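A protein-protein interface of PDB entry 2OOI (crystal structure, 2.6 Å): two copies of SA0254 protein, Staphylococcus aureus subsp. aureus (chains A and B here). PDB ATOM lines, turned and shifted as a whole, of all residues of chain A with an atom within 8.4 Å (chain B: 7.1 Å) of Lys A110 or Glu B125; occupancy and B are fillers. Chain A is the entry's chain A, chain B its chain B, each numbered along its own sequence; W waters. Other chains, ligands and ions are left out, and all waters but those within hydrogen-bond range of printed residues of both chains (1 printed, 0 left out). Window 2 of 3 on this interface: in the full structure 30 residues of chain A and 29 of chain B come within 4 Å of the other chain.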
ATOM      1  N   ASN A 107     -12.666  -0.403   9.801  1.00  0.00           N
ATOM      2  CA  ASN A 107     -12.517  -0.435   8.360  1.00  0.00           C
ATOM      3  C   ASN A 107     -12.909  -1.810   7.864  1.00  0.00           C
ATOM      4  O   ASN A 107     -12.966  -2.778   8.652  1.00  0.00           O
ATOM      5  CB  ASN A 107     -11.072  -0.119   7.954  1.00  0.00           C
ATOM      6  CG  ASN A 107     -10.079  -1.177   8.438  1.00  0.00           C
ATOM      7  OD1 ASN A 107     -10.466  -2.184   9.066  1.00  0.00           O
ATOM      8  ND2 ASN A 107      -8.794  -0.954   8.148  1.00  0.00           N
ATOM      9  N   VAL A 108     -13.151  -1.897   6.566  1.00  0.00           N
ATOM     10  CA  VAL A 108     -13.533  -3.142   5.946  1.00  0.00           C
ATOM     11  C   VAL A 108     -12.251  -3.732   5.380  1.00  0.00           C
ATOM     12  O   VAL A 108     -11.365  -2.998   4.962  1.00  0.00           O
ATOM     13  CB  VAL A 108     -14.601  -2.902   4.826  1.00  0.00           C
ATOM     14  CG1 VAL A 108     -14.740  -4.120   3.929  1.00  0.00           C
ATOM     15  CG2 VAL A 108     -15.936  -2.494   5.450  1.00  0.00           C
ATOM     16  N   ASP A 109     -12.162  -5.053   5.339  1.00  0.00           N
ATOM     17  CA  ASP A 109     -10.969  -5.715   4.846  1.00  0.00           C
ATOM     18  C   ASP A 109     -11.298  -7.118   4.357  1.00  0.00           C
ATOM     19  O   ASP A 109     -12.434  -7.569   4.491  1.00  0.00           O
ATOM     20  CB  ASP A 109      -9.946  -5.816   5.990  1.00  0.00           C
ATOM     21  CG  ASP A 109      -8.509  -5.903   5.504  1.00  0.00           C
ATOM     22  OD1 ASP A 109      -8.235  -6.034   4.307  1.00  0.00           O
ATOM     23  OD2 ASP A 109      -7.613  -5.818   6.336  1.00  0.00           O
ATOM     24  N   LYS A 110     -10.276  -7.796   3.827  1.00  0.00           N
ATOM     25  CA  LYS A 110     -10.338  -9.202   3.482  1.00  0.00           C
ATOM     26  C   LYS A 110      -9.951  -9.998   4.704  1.00  0.00           C
ATOM     27  O   LYS A 110      -9.166  -9.531   5.513  1.00  0.00           O
ATOM     28  CB  LYS A 110      -9.365  -9.534   2.356  1.00  0.00           C
ATOM     29  CG  LYS A 110      -9.378  -8.534   1.230  1.00  0.00           C
ATOM     30  CD  LYS A 110      -8.803  -9.076  -0.075  1.00  0.00           C
ATOM     31  CE  LYS A 110      -9.156  -8.167  -1.250  1.00  0.00           C
ATOM     32  NZ  LYS A 110      -8.929  -8.811  -2.551  1.00  0.00           N
ATOM     33  N   LEU A 111     -10.501 -11.204   4.827  1.00  0.00           N
ATOM     34  CA  LEU A 111     -10.195 -12.066   5.954  1.00  0.00           C
ATOM     35  C   LEU A 111      -8.931 -12.796   5.665  1.00  0.00           C
ATOM     36  O   LEU A 111      -8.549 -13.067   4.541  1.00  0.00           O
ATOM     37  CB  LEU A 111     -11.261 -13.139   6.190  1.00  0.00           C
ATOM     38  CG  LEU A 111     -12.647 -12.787   6.721  1.00  0.00           C
ATOM     39  CD1 LEU A 111     -13.597 -13.837   6.200  1.00  0.00           C
ATOM     40  CD2 LEU A 111     -12.669 -12.694   8.243  1.00  0.00           C
ATOM     41  N   THR A 112      -8.306 -13.172   6.729  1.00  0.00           N
ATOM     42  CA  THR A 112      -7.131 -13.970   6.667  1.00  0.00           C
ATOM     43  C   THR A 112      -7.601 -15.413   6.489  1.00  0.00           C
ATOM     44  O   THR A 112      -8.807 -15.683   6.427  1.00  0.00           O
ATOM     45  CB  THR A 112      -6.339 -13.680   7.964  1.00  0.00           C
ATOM     46  OG1 THR A 112      -6.019 -12.294   7.989  1.00  0.00           O
ATOM     47  CG2 THR A 112      -5.157 -14.562   8.166  1.00  0.00           C
ATOM     48  N   SER A 113      -6.653 -16.325   6.365  1.00  0.00           N
ATOM     49  CA  SER A 113      -6.937 -17.748   6.236  1.00  0.00           C
ATOM     50  C   SER A 113      -7.499 -18.299   7.529  1.00  0.00           C
ATOM     51  O   SER A 113      -8.489 -19.010   7.538  1.00  0.00           O
ATOM     52  CB  SER A 113      -5.642 -18.491   5.894  1.00  0.00           C
ATOM     53  OG  SER A 113      -5.925 -19.653   5.146  1.00  0.00           O
ATOM     54  N   GLU A 115      -8.740 -16.581  10.061  1.00  0.00           N
ATOM     55  CA  GLU A 115      -9.955 -15.854  10.440  1.00  0.00           C
ATOM     56  C   GLU A 115     -11.157 -16.423   9.703  1.00  0.00           C
ATOM     57  O   GLU A 115     -12.171 -16.725  10.325  1.00  0.00           O
ATOM     58  CB  GLU A 115      -9.817 -14.380  10.105  1.00  0.00           C
ATOM     59  CG  GLU A 115      -8.810 -13.655  10.933  1.00  0.00           C
ATOM     60  CD  GLU A 115      -8.425 -12.334  10.337  1.00  0.00           C
ATOM     61  OE1 GLU A 115      -8.724 -12.106   9.156  1.00  0.00           O
ATOM     62  OE2 GLU A 115      -7.810 -11.518  11.043  1.00  0.00           O
ATOM     63  N   ALA A 116     -11.022 -16.581   8.387  1.00  0.00           N
ATOM     64  CA  ALA A 116     -12.058 -17.221   7.586  1.00  0.00           C
ATOM     65  C   ALA A 116     -12.374 -18.590   8.182  1.00  0.00           C
ATOM     66  O   ALA A 116     -13.522 -19.007   8.234  1.00  0.00           O
ATOM     67  CB  ALA A 116     -11.628 -17.346   6.094  1.00  0.00           C
ATOM     68  N   SER A 122     -14.571 -18.275   3.617  1.00  0.00           N
ATOM     69  CA  SER A 122     -13.387 -18.514   2.764  1.00  0.00           C
ATOM     70  C   SER A 122     -12.350 -17.381   2.895  1.00  0.00           C
ATOM     71  O   SER A 122     -12.723 -16.180   2.911  1.00  0.00           O
ATOM     72  CB  SER A 122     -13.770 -18.577   1.266  1.00  0.00           C
ATOM     73  OG  SER A 122     -15.078 -19.073   1.034  1.00  0.00           O
ATOM     74  N   THR A 123     -11.066 -17.765   2.922  1.00  0.00           N
ATOM     75  CA  THR A 123      -9.933 -16.830   2.803  1.00  0.00           C
ATOM     76  C   THR A 123     -10.244 -15.687   1.847  1.00  0.00           C
ATOM     77  O   THR A 123     -10.741 -15.914   0.736  1.00  0.00           O
ATOM     78  CB  THR A 123      -8.663 -17.561   2.301  1.00  0.00           C
ATOM     79  OG1 THR A 123      -8.047 -18.241   3.398  1.00  0.00           O
ATOM     80  CG2 THR A 123      -7.652 -16.595   1.714  1.00  0.00           C
ATOM     81  N   GLY A 124      -9.979 -14.457   2.283  1.00  0.00           N
ATOM     82  CA  GLY A 124     -10.162 -13.291   1.413  1.00  0.00           C
ATOM     83  C   GLY A 124     -11.550 -12.672   1.324  1.00  0.00           C
ATOM     84  O   GLY A 124     -11.688 -11.603   0.747  1.00  0.00           O
ATOM     85  N   GLU A 125     -12.582 -13.311   1.873  1.00  0.00           N
ATOM     86  CA  GLU A 125     -13.918 -12.693   1.912  1.00  0.00           C
ATOM     87  C   GLU A 125     -13.977 -11.493   2.879  1.00  0.00           C
ATOM     88  O   GLU A 125     -13.155 -11.375   3.817  1.00  0.00           O
ATOM     89  CB  GLU A 125     -14.995 -13.710   2.318  1.00  0.00           C
ATOM     90  CG  GLU A 125     -15.145 -14.877   1.348  1.00  0.00           C
ATOM     91  CD  GLU A 125     -16.437 -15.635   1.556  1.00  0.00           C
ATOM     92  OE1 GLU A 125     -16.446 -16.609   2.400  1.00  0.00           O
ATOM     93  OE2 GLU A 125     -17.433 -15.240   0.846  1.00  0.00           O
ATOM     94  N   PRO A 126     -14.976 -10.620   2.688  1.00  0.00           N
ATOM     95  CA  PRO A 126     -15.019  -9.407   3.466  1.00  0.00           C
ATOM     96  C   PRO A 126     -15.164  -9.644   4.958  1.00  0.00           C
ATOM     97  O   PRO A 126     -15.608 -10.701   5.392  1.00  0.00           O
ATOM     98  CB  PRO A 126     -16.282  -8.704   2.944  1.00  0.00           C
ATOM     99  CG  PRO A 126     -16.521  -9.276   1.627  1.00  0.00           C
ATOM    100  CD  PRO A 126     -16.126 -10.699   1.770  1.00  0.00           C
ATOM    101  N   CYS A 127     -14.787  -8.636   5.725  1.00  0.00           N
ATOM    102  CA  CYS A 127     -15.010  -8.621   7.163  1.00  0.00           C
ATOM    103  C   CYS A 127     -14.928  -7.163   7.586  1.00  0.00           C
ATOM    104  O   CYS A 127     -14.542  -6.322   6.789  1.00  0.00           O
ATOM    105  CB  CYS A 127     -13.942  -9.435   7.888  1.00  0.00           C
ATOM    106  SG  CYS A 127     -12.275  -8.715   7.763  1.00  0.00           S
ATOM    107  N   LEU A 128     -15.326  -6.881   8.825  1.00  0.00           N
ATOM    108  CA  LEU A 128     -15.142  -5.586   9.444  1.00  0.00           C
ATOM    109  C   LEU A 128     -14.087  -5.727  10.536  1.00  0.00           C
ATOM    110  O   LEU A 128     -14.211  -6.603  11.400  1.00  0.00           O
ATOM    111  CB  LEU A 128     -16.441  -5.102  10.074  1.00  0.00           C
ATOM    112  CG  LEU A 128     -16.372  -3.606  10.423  1.00  0.00           C
ATOM    113  CD1 LEU A 128     -16.407  -2.739   9.102  1.00  0.00           C
ATOM    114  CD2 LEU A 128     -17.453  -3.184  11.407  1.00  0.00           C
ATOM    115  N   ARG A 129     -13.069  -4.862  10.516  1.00  0.00           N
ATOM    116  CA  ARG A 129     -12.092  -4.792  11.647  1.00  0.00           C
ATOM    117  C   ARG A 129     -12.488  -3.627  12.501  1.00  0.00           C
ATOM    118  O   ARG A 129     -12.654  -2.522  12.014  1.00  0.00           O
ATOM    119  CB  ARG A 129     -10.644  -4.677  11.187  1.00  0.00           C
ATOM    120  CG  ARG A 129     -10.349  -5.690  10.122  1.00  0.00           C
ATOM    121  CD  ARG A 129      -8.898  -5.856   9.734  1.00  0.00           C
ATOM    122  NE  ARG A 129      -8.693  -7.285   9.925  1.00  0.00           N
ATOM    123  CZ  ARG A 129      -8.384  -8.166   8.993  1.00  0.00           C
ATOM    124  NH1 ARG A 129      -8.105  -7.792   7.776  1.00  0.00           N
ATOM    125  NH2 ARG A 129      -8.303  -9.431   9.310  1.00  0.00           N
ATOM    126  N   VAL A 148     -13.079  -8.934  14.780  1.00  0.00           N
ATOM    127  CA  VAL A 148     -13.291  -9.065  13.363  1.00  0.00           C
ATOM    128  C   VAL A 148     -14.652  -9.695  13.215  1.00  0.00           C
ATOM    129  O   VAL A 148     -14.890 -10.769  13.728  1.00  0.00           O
ATOM    130  CB  VAL A 148     -12.142  -9.764  12.598  1.00  0.00           C
ATOM    131  CG1 VAL A 148     -12.490  -9.956  11.103  1.00  0.00           C
ATOM    132  CG2 VAL A 148     -10.839  -9.073  12.829  1.00  0.00           C
ATOM    133  N   ASP B 109     -20.225  -6.024   2.763  1.00  0.00           N
ATOM    134  CA  ASP B 109     -20.710  -6.873   1.667  1.00  0.00           C
ATOM    135  C   ASP B 109     -19.629  -6.969   0.580  1.00  0.00           C
ATOM    136  O   ASP B 109     -18.544  -6.375   0.713  1.00  0.00           O
ATOM    137  CB  ASP B 109     -22.003  -6.279   1.080  1.00  0.00           C
ATOM    138  CG  ASP B 109     -22.863  -7.302   0.288  1.00  0.00           C
ATOM    139  OD1 ASP B 109     -22.481  -8.484   0.109  1.00  0.00           O
ATOM    140  OD2 ASP B 109     -23.970  -6.908  -0.174  1.00  0.00           O
ATOM    141  N   LYS B 110     -19.933  -7.732  -0.474  1.00  0.00           N
ATOM    142  CA  LYS B 110     -19.120  -7.821  -1.659  1.00  0.00           C
ATOM    143  C   LYS B 110     -19.584  -6.789  -2.664  1.00  0.00           C
ATOM    144  O   LYS B 110     -20.715  -6.382  -2.624  1.00  0.00           O
ATOM    145  CB  LYS B 110     -19.279  -9.188  -2.277  1.00  0.00           C
ATOM    146  CG  LYS B 110     -18.759 -10.273  -1.433  1.00  0.00           C
ATOM    147  CD  LYS B 110     -18.593 -11.570  -2.204  1.00  0.00           C
ATOM    148  CE  LYS B 110     -18.448 -12.746  -1.224  1.00  0.00           C
ATOM    149  NZ  LYS B 110     -17.979 -13.994  -1.891  1.00  0.00           N
ATOM    150  N   LEU B 111     -18.703  -6.388  -3.571  1.00  0.00           N
ATOM    151  CA  LEU B 111     -19.014  -5.400  -4.582  1.00  0.00           C
ATOM    152  C   LEU B 111     -19.668  -6.019  -5.823  1.00  0.00           C
ATOM    153  O   LEU B 111     -19.369  -7.147  -6.240  1.00  0.00           O
ATOM    154  CB  LEU B 111     -17.742  -4.693  -5.038  1.00  0.00           C
ATOM    155  CG  LEU B 111     -17.125  -3.580  -4.206  1.00  0.00           C
ATOM    156  CD1 LEU B 111     -15.748  -3.373  -4.772  1.00  0.00           C
ATOM    157  CD2 LEU B 111     -17.947  -2.293  -4.242  1.00  0.00           C
ATOM    158  N   THR B 112     -20.541  -5.254  -6.440  1.00  0.00           N
ATOM    159  CA  THR B 112     -21.071  -5.659  -7.713  1.00  0.00           C
ATOM    160  C   THR B 112     -20.016  -5.262  -8.726  1.00  0.00           C
ATOM    161  O   THR B 112     -19.147  -4.432  -8.437  1.00  0.00           O
ATOM    162  CB  THR B 112     -22.385  -4.953  -8.029  1.00  0.00           C
ATOM    163  OG1 THR B 112     -22.112  -3.579  -8.345  1.00  0.00           O
ATOM    164  CG2 THR B 112     -23.384  -5.067  -6.834  1.00  0.00           C
ATOM    165  N   GLU B 115     -20.261  -1.421  -9.428  1.00  0.00           N
ATOM    166  CA  GLU B 115     -19.603  -0.698  -8.331  1.00  0.00           C
ATOM    167  C   GLU B 115     -18.073  -0.844  -8.358  1.00  0.00           C
ATOM    168  O   GLU B 115     -17.344   0.123  -8.088  1.00  0.00           O
ATOM    169  CB  GLU B 115     -20.102  -1.198  -7.003  1.00  0.00           C
ATOM    170  CG  GLU B 115     -21.540  -0.839  -6.718  1.00  0.00           C
ATOM    171  CD  GLU B 115     -22.200  -1.818  -5.760  1.00  0.00           C
ATOM    172  OE1 GLU B 115     -21.552  -2.815  -5.319  1.00  0.00           O
ATOM    173  OE2 GLU B 115     -23.398  -1.598  -5.476  1.00  0.00           O
ATOM    174  N   ALA B 116     -17.583  -2.039  -8.676  1.00  0.00           N
ATOM    175  CA  ALA B 116     -16.131  -2.271  -8.656  1.00  0.00           C
ATOM    176  C   ALA B 116     -15.444  -1.407  -9.698  1.00  0.00           C
ATOM    177  O   ALA B 116     -14.356  -0.900  -9.467  1.00  0.00           O
ATOM    178  CB  ALA B 116     -15.789  -3.758  -8.863  1.00  0.00           C
ATOM    179  N   GLN B 120     -12.686   1.404  -9.030  1.00  0.00           N
ATOM    180  CA  GLN B 120     -11.389   0.871  -9.456  1.00  0.00           C
ATOM    181  C   GLN B 120     -10.866  -0.261  -8.558  1.00  0.00           C
ATOM    182  O   GLN B 120      -9.721  -0.208  -8.052  1.00  0.00           O
ATOM    183  CB  GLN B 120     -10.377   1.994  -9.506  1.00  0.00           C
ATOM    184  CG  GLN B 120     -10.708   3.025 -10.542  1.00  0.00           C
ATOM    185  CD  GLN B 120      -9.610   4.039 -10.622  1.00  0.00           C
ATOM    186  OE1 GLN B 120      -8.648   3.877 -11.385  1.00  0.00           O
ATOM    187  NE2 GLN B 120      -9.695   5.059  -9.765  1.00  0.00           N
ATOM    188  N   LEU B 121     -11.740  -1.257  -8.369  1.00  0.00           N
ATOM    189  CA  LEU B 121     -11.478  -2.474  -7.605  1.00  0.00           C
ATOM    190  C   LEU B 121     -12.044  -3.629  -8.434  1.00  0.00           C
ATOM    191  O   LEU B 121     -12.556  -3.399  -9.528  1.00  0.00           O
ATOM    192  CB  LEU B 121     -12.165  -2.388  -6.232  1.00  0.00           C
ATOM    193  CG  LEU B 121     -11.496  -1.405  -5.241  1.00  0.00           C
ATOM    194  CD1 LEU B 121     -12.339  -1.052  -3.985  1.00  0.00           C
ATOM    195  CD2 LEU B 121     -10.106  -1.937  -4.839  1.00  0.00           C
ATOM    196  N   SER B 122     -11.998  -4.855  -7.905  1.00  0.00           N
ATOM    197  CA  SER B 122     -12.532  -6.031  -8.633  1.00  0.00           C
ATOM    198  C   SER B 122     -13.904  -6.476  -8.122  1.00  0.00           C
ATOM    199  O   SER B 122     -14.141  -6.455  -6.902  1.00  0.00           O
ATOM    200  CB  SER B 122     -11.578  -7.208  -8.481  1.00  0.00           C
ATOM    201  OG  SER B 122     -10.245  -6.797  -8.690  1.00  0.00           O
ATOM    202  N   THR B 123     -14.769  -6.930  -9.041  1.00  0.00           N
ATOM    203  CA  THR B 123     -16.022  -7.597  -8.667  1.00  0.00           C
ATOM    204  C   THR B 123     -15.817  -8.538  -7.481  1.00  0.00           C
ATOM    205  O   THR B 123     -14.926  -9.396  -7.507  1.00  0.00           O
ATOM    206  CB  THR B 123     -16.622  -8.444  -9.825  1.00  0.00           C
ATOM    207  OG1 THR B 123     -16.888  -7.602 -10.954  1.00  0.00           O
ATOM    208  CG2 THR B 123     -17.948  -9.121  -9.401  1.00  0.00           C
ATOM    209  N   GLY B 124     -16.638  -8.368  -6.448  1.00  0.00           N
ATOM    210  CA  GLY B 124     -16.602  -9.275  -5.306  1.00  0.00           C
ATOM    211  C   GLY B 124     -15.688  -8.859  -4.168  1.00  0.00           C
ATOM    212  O   GLY B 124     -15.771  -9.400  -3.080  1.00  0.00           O
ATOM    213  N   GLU B 125     -14.804  -7.902  -4.409  1.00  0.00           N
ATOM    214  CA  GLU B 125     -13.974  -7.388  -3.330  1.00  0.00           C
ATOM    215  C   GLU B 125     -14.826  -6.618  -2.324  1.00  0.00           C
ATOM    216  O   GLU B 125     -15.876  -6.079  -2.684  1.00  0.00           O
ATOM    217  CB  GLU B 125     -12.867  -6.494  -3.879  1.00  0.00           C
ATOM    218  CG  GLU B 125     -11.704  -7.271  -4.433  1.00  0.00           C
ATOM    219  CD  GLU B 125     -10.555  -6.391  -4.769  1.00  0.00           C
ATOM    220  OE1 GLU B 125     -10.757  -5.408  -5.527  1.00  0.00           O
ATOM    221  OE2 GLU B 125      -9.451  -6.698  -4.265  1.00  0.00           O
ATOM    222  N   PRO B 126     -14.373  -6.545  -1.074  1.00  0.00           N
ATOM    223  CA  PRO B 126     -15.206  -6.020  -0.008  1.00  0.00           C
ATOM    224  C   PRO B 126     -15.593  -4.540  -0.144  1.00  0.00           C
ATOM    225  O   PRO B 126     -14.887  -3.753  -0.798  1.00  0.00           O
ATOM    226  CB  PRO B 126     -14.334  -6.199   1.244  1.00  0.00           C
ATOM    227  CG  PRO B 126     -13.252  -7.157   0.863  1.00  0.00           C
ATOM    228  CD  PRO B 126     -13.045  -6.938  -0.599  1.00  0.00           C
ATOM    229  N   CYS B 127     -16.716  -4.175   0.477  1.00  0.00           N
ATOM    230  CA  CYS B 127     -17.125  -2.763   0.601  1.00  0.00           C
ATOM    231  C   CYS B 127     -17.885  -2.569   1.908  1.00  0.00           C
ATOM    232  O   CYS B 127     -18.160  -3.544   2.603  1.00  0.00           O
ATOM    233  CB  CYS B 127     -18.015  -2.356  -0.577  1.00  0.00           C
ATOM    234  SG  CYS B 127     -19.474  -3.446  -0.795  1.00  0.00           S
ATOM    235  N   TYR B 151     -13.116   0.030   0.119  1.00  0.00           N
ATOM    236  CA  TYR B 151     -12.731  -0.572   1.387  1.00  0.00           C
ATOM    237  C   TYR B 151     -11.347  -0.207   1.914  1.00  0.00           C
ATOM    238  O   TYR B 151     -11.126  -0.286   3.124  1.00  0.00           O
ATOM    239  CB  TYR B 151     -12.918  -2.077   1.370  1.00  0.00           C
ATOM    240  CG  TYR B 151     -11.792  -2.853   0.774  1.00  0.00           C
ATOM    241  CD1 TYR B 151     -10.891  -3.518   1.583  1.00  0.00           C
ATOM    242  CD2 TYR B 151     -11.636  -2.948  -0.604  1.00  0.00           C
ATOM    243  CE1 TYR B 151      -9.854  -4.231   1.040  1.00  0.00           C
ATOM    244  CE2 TYR B 151     -10.618  -3.671  -1.148  1.00  0.00           C
ATOM    245  CZ  TYR B 151      -9.727  -4.308  -0.320  1.00  0.00           C
ATOM    246  OH  TYR B 151      -8.698  -5.036  -0.843  1.00  0.00           O
ATOM    247  N   ARG B 152     -10.424   0.156   1.029  1.00  0.00           N
ATOM    248  CA  ARG B 152      -9.081   0.592   1.435  1.00  0.00           C
ATOM    249  C   ARG B 152      -9.039   2.072   1.804  1.00  0.00           C
ATOM    250  O   ARG B 152      -8.395   2.448   2.769  1.00  0.00           O
ATOM    251  CB  ARG B 152      -8.040   0.326   0.344  1.00  0.00           C
ATOM    252  CG  ARG B 152      -7.749  -1.141   0.075  1.00  0.00           C
ATOM    253  CD  ARG B 152      -6.694  -1.350  -1.065  1.00  0.00           C
ATOM    254  NE  ARG B 152      -6.477  -2.786  -1.291  1.00  0.00           N
ATOM    255  CZ  ARG B 152      -5.696  -3.351  -2.235  1.00  0.00           C
ATOM    256  NH1 ARG B 152      -4.922  -2.625  -3.071  1.00  0.00           N
ATOM    257  NH2 ARG B 152      -5.657  -4.687  -2.325  1.00  0.00           N
HETATM  258  O   HOH W   1     -12.889   0.269   5.000  1.00  0.00           O
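O of Tyr B151 sits close to O of Val A108.
NZ of Lys B110 is in salt-bridge range of OE2 of Glu A125 (3.1 Å).
NZ of Lys A110 lies within salt-bridge range of OE2 of Glu B125, at 2.8 Å.
N of Ser A122 lies within hydrogen-bond range of OE1 of Glu A125, at 2.8 Å.
OD2 of Asp A109 lies within salt-bridge range of NH1 of Arg A129, 2.5 Å away.
The backbone NH of Leu B111 sits at hydrogen-bond distance from the backbone carbonyl oxygen of Glu B125 (3.0 Å).
O of Asp A109 is in hydrogen-bond range of N of Cys A127.
The backbone NH (N) of Leu A111 lies within hydrogen-bond range of the backbone carbonyl oxygen (O) of Glu A125 (2.8 Å).
The backbone carbonyl oxygen of Asp B109 sits at hydrogen-bond distance from the backbone NH of Cys B127 (2.9 Å).
Pro B126 touches Val A108 (CB to CG1, 3.4 Å).
Cys B127 touches Val A108 (O to CG1, 3.7 Å).
CG of Pro B126 touches O of Asp A109 (3.7 Å).
CA of Asp A109 touches CD1 of Tyr B151, at 3.9 Å.
Lys A110 touches Tyr B151 (CE to OH, 3.2 Å).
Asp B109 touches Pro A126 (O to CG, 3.7 Å).
Pro A126 touches Lys B110.
Pro A126 touches Pro B126 (CB to CB, 3.6 Å).
Asn A107 touches none of the printed residues of chain B.
Printed residues of chain B within 4 Å of Asp A109: Pro B126 (3.7 Å) and Tyr B151 (3.9 Å).
Of chain B, only Glu B125 and Tyr B151 come within 4 Å of Lys A110.
Of the printed residues of chain B, Glu A125 touches Lys B110.
Of the printed residues of chain B, Pro A126 touches Asp B109, Lys B110 and Pro B126.
Leu A128 touches none of the printed residues of chain B.
Printed residues of chain A within 4 Å of Asp B109: Pro A126.
Gly B124 touches none of the printed residues of chain A.
Of chain A, only Lys A110 comes within 4 Å of Glu B125.
Of the printed residues of chain A, Pro B126 touches Val A108, Asp A109 and Pro A126.
Of the printed residues of chain A, Cys B127 touches Val A108.
The nearest printed residue of chain A that does not touch Asp B109 is Val A108 (5.5 Å).
Printed residues of chain B that touch a printed residue of chain A: Asp B109, Lys B110, Glu B125, Pro B126, Cys B127 and Tyr B151.
Printed residues of chain A that touch a printed residue of chain B: Val A108, Asp A109, Lys A110, Glu A125 and Pro A126.
Hydrophobic or aromatic side chains of chain A that line the printed part of chain B: Val A108 and Pro A126.
Among the printed residues, Asp or Glu carboxylates within 4 Å of a Lys or Arg side-chain nitrogen of the other chain: Lys A110 with Glu B125 (2.8 Å) and Glu A125 with Lys B110 (3.1 Å).
Asp A109 touches Pro B126, and with the chains exchanged Pro A126 touches Asp B109.
Lys A110 touches Glu B125, and with the chains exchanged Glu A125 touches Lys B110.
Pro A126 touches Lys B110, but with the chains exchanged Lys A110 does not touch Pro B126 (4.1 Å).
Pro A126 touches its own counterpart, Pro B126.
Positions printed for both chains: 109, 110, 111, 112, 115, 116, 122, 123, 124, 125, 126 and 127.
Water W1 lies within hydrogen-bond range of O of Tyr B151 and N of Val A108.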
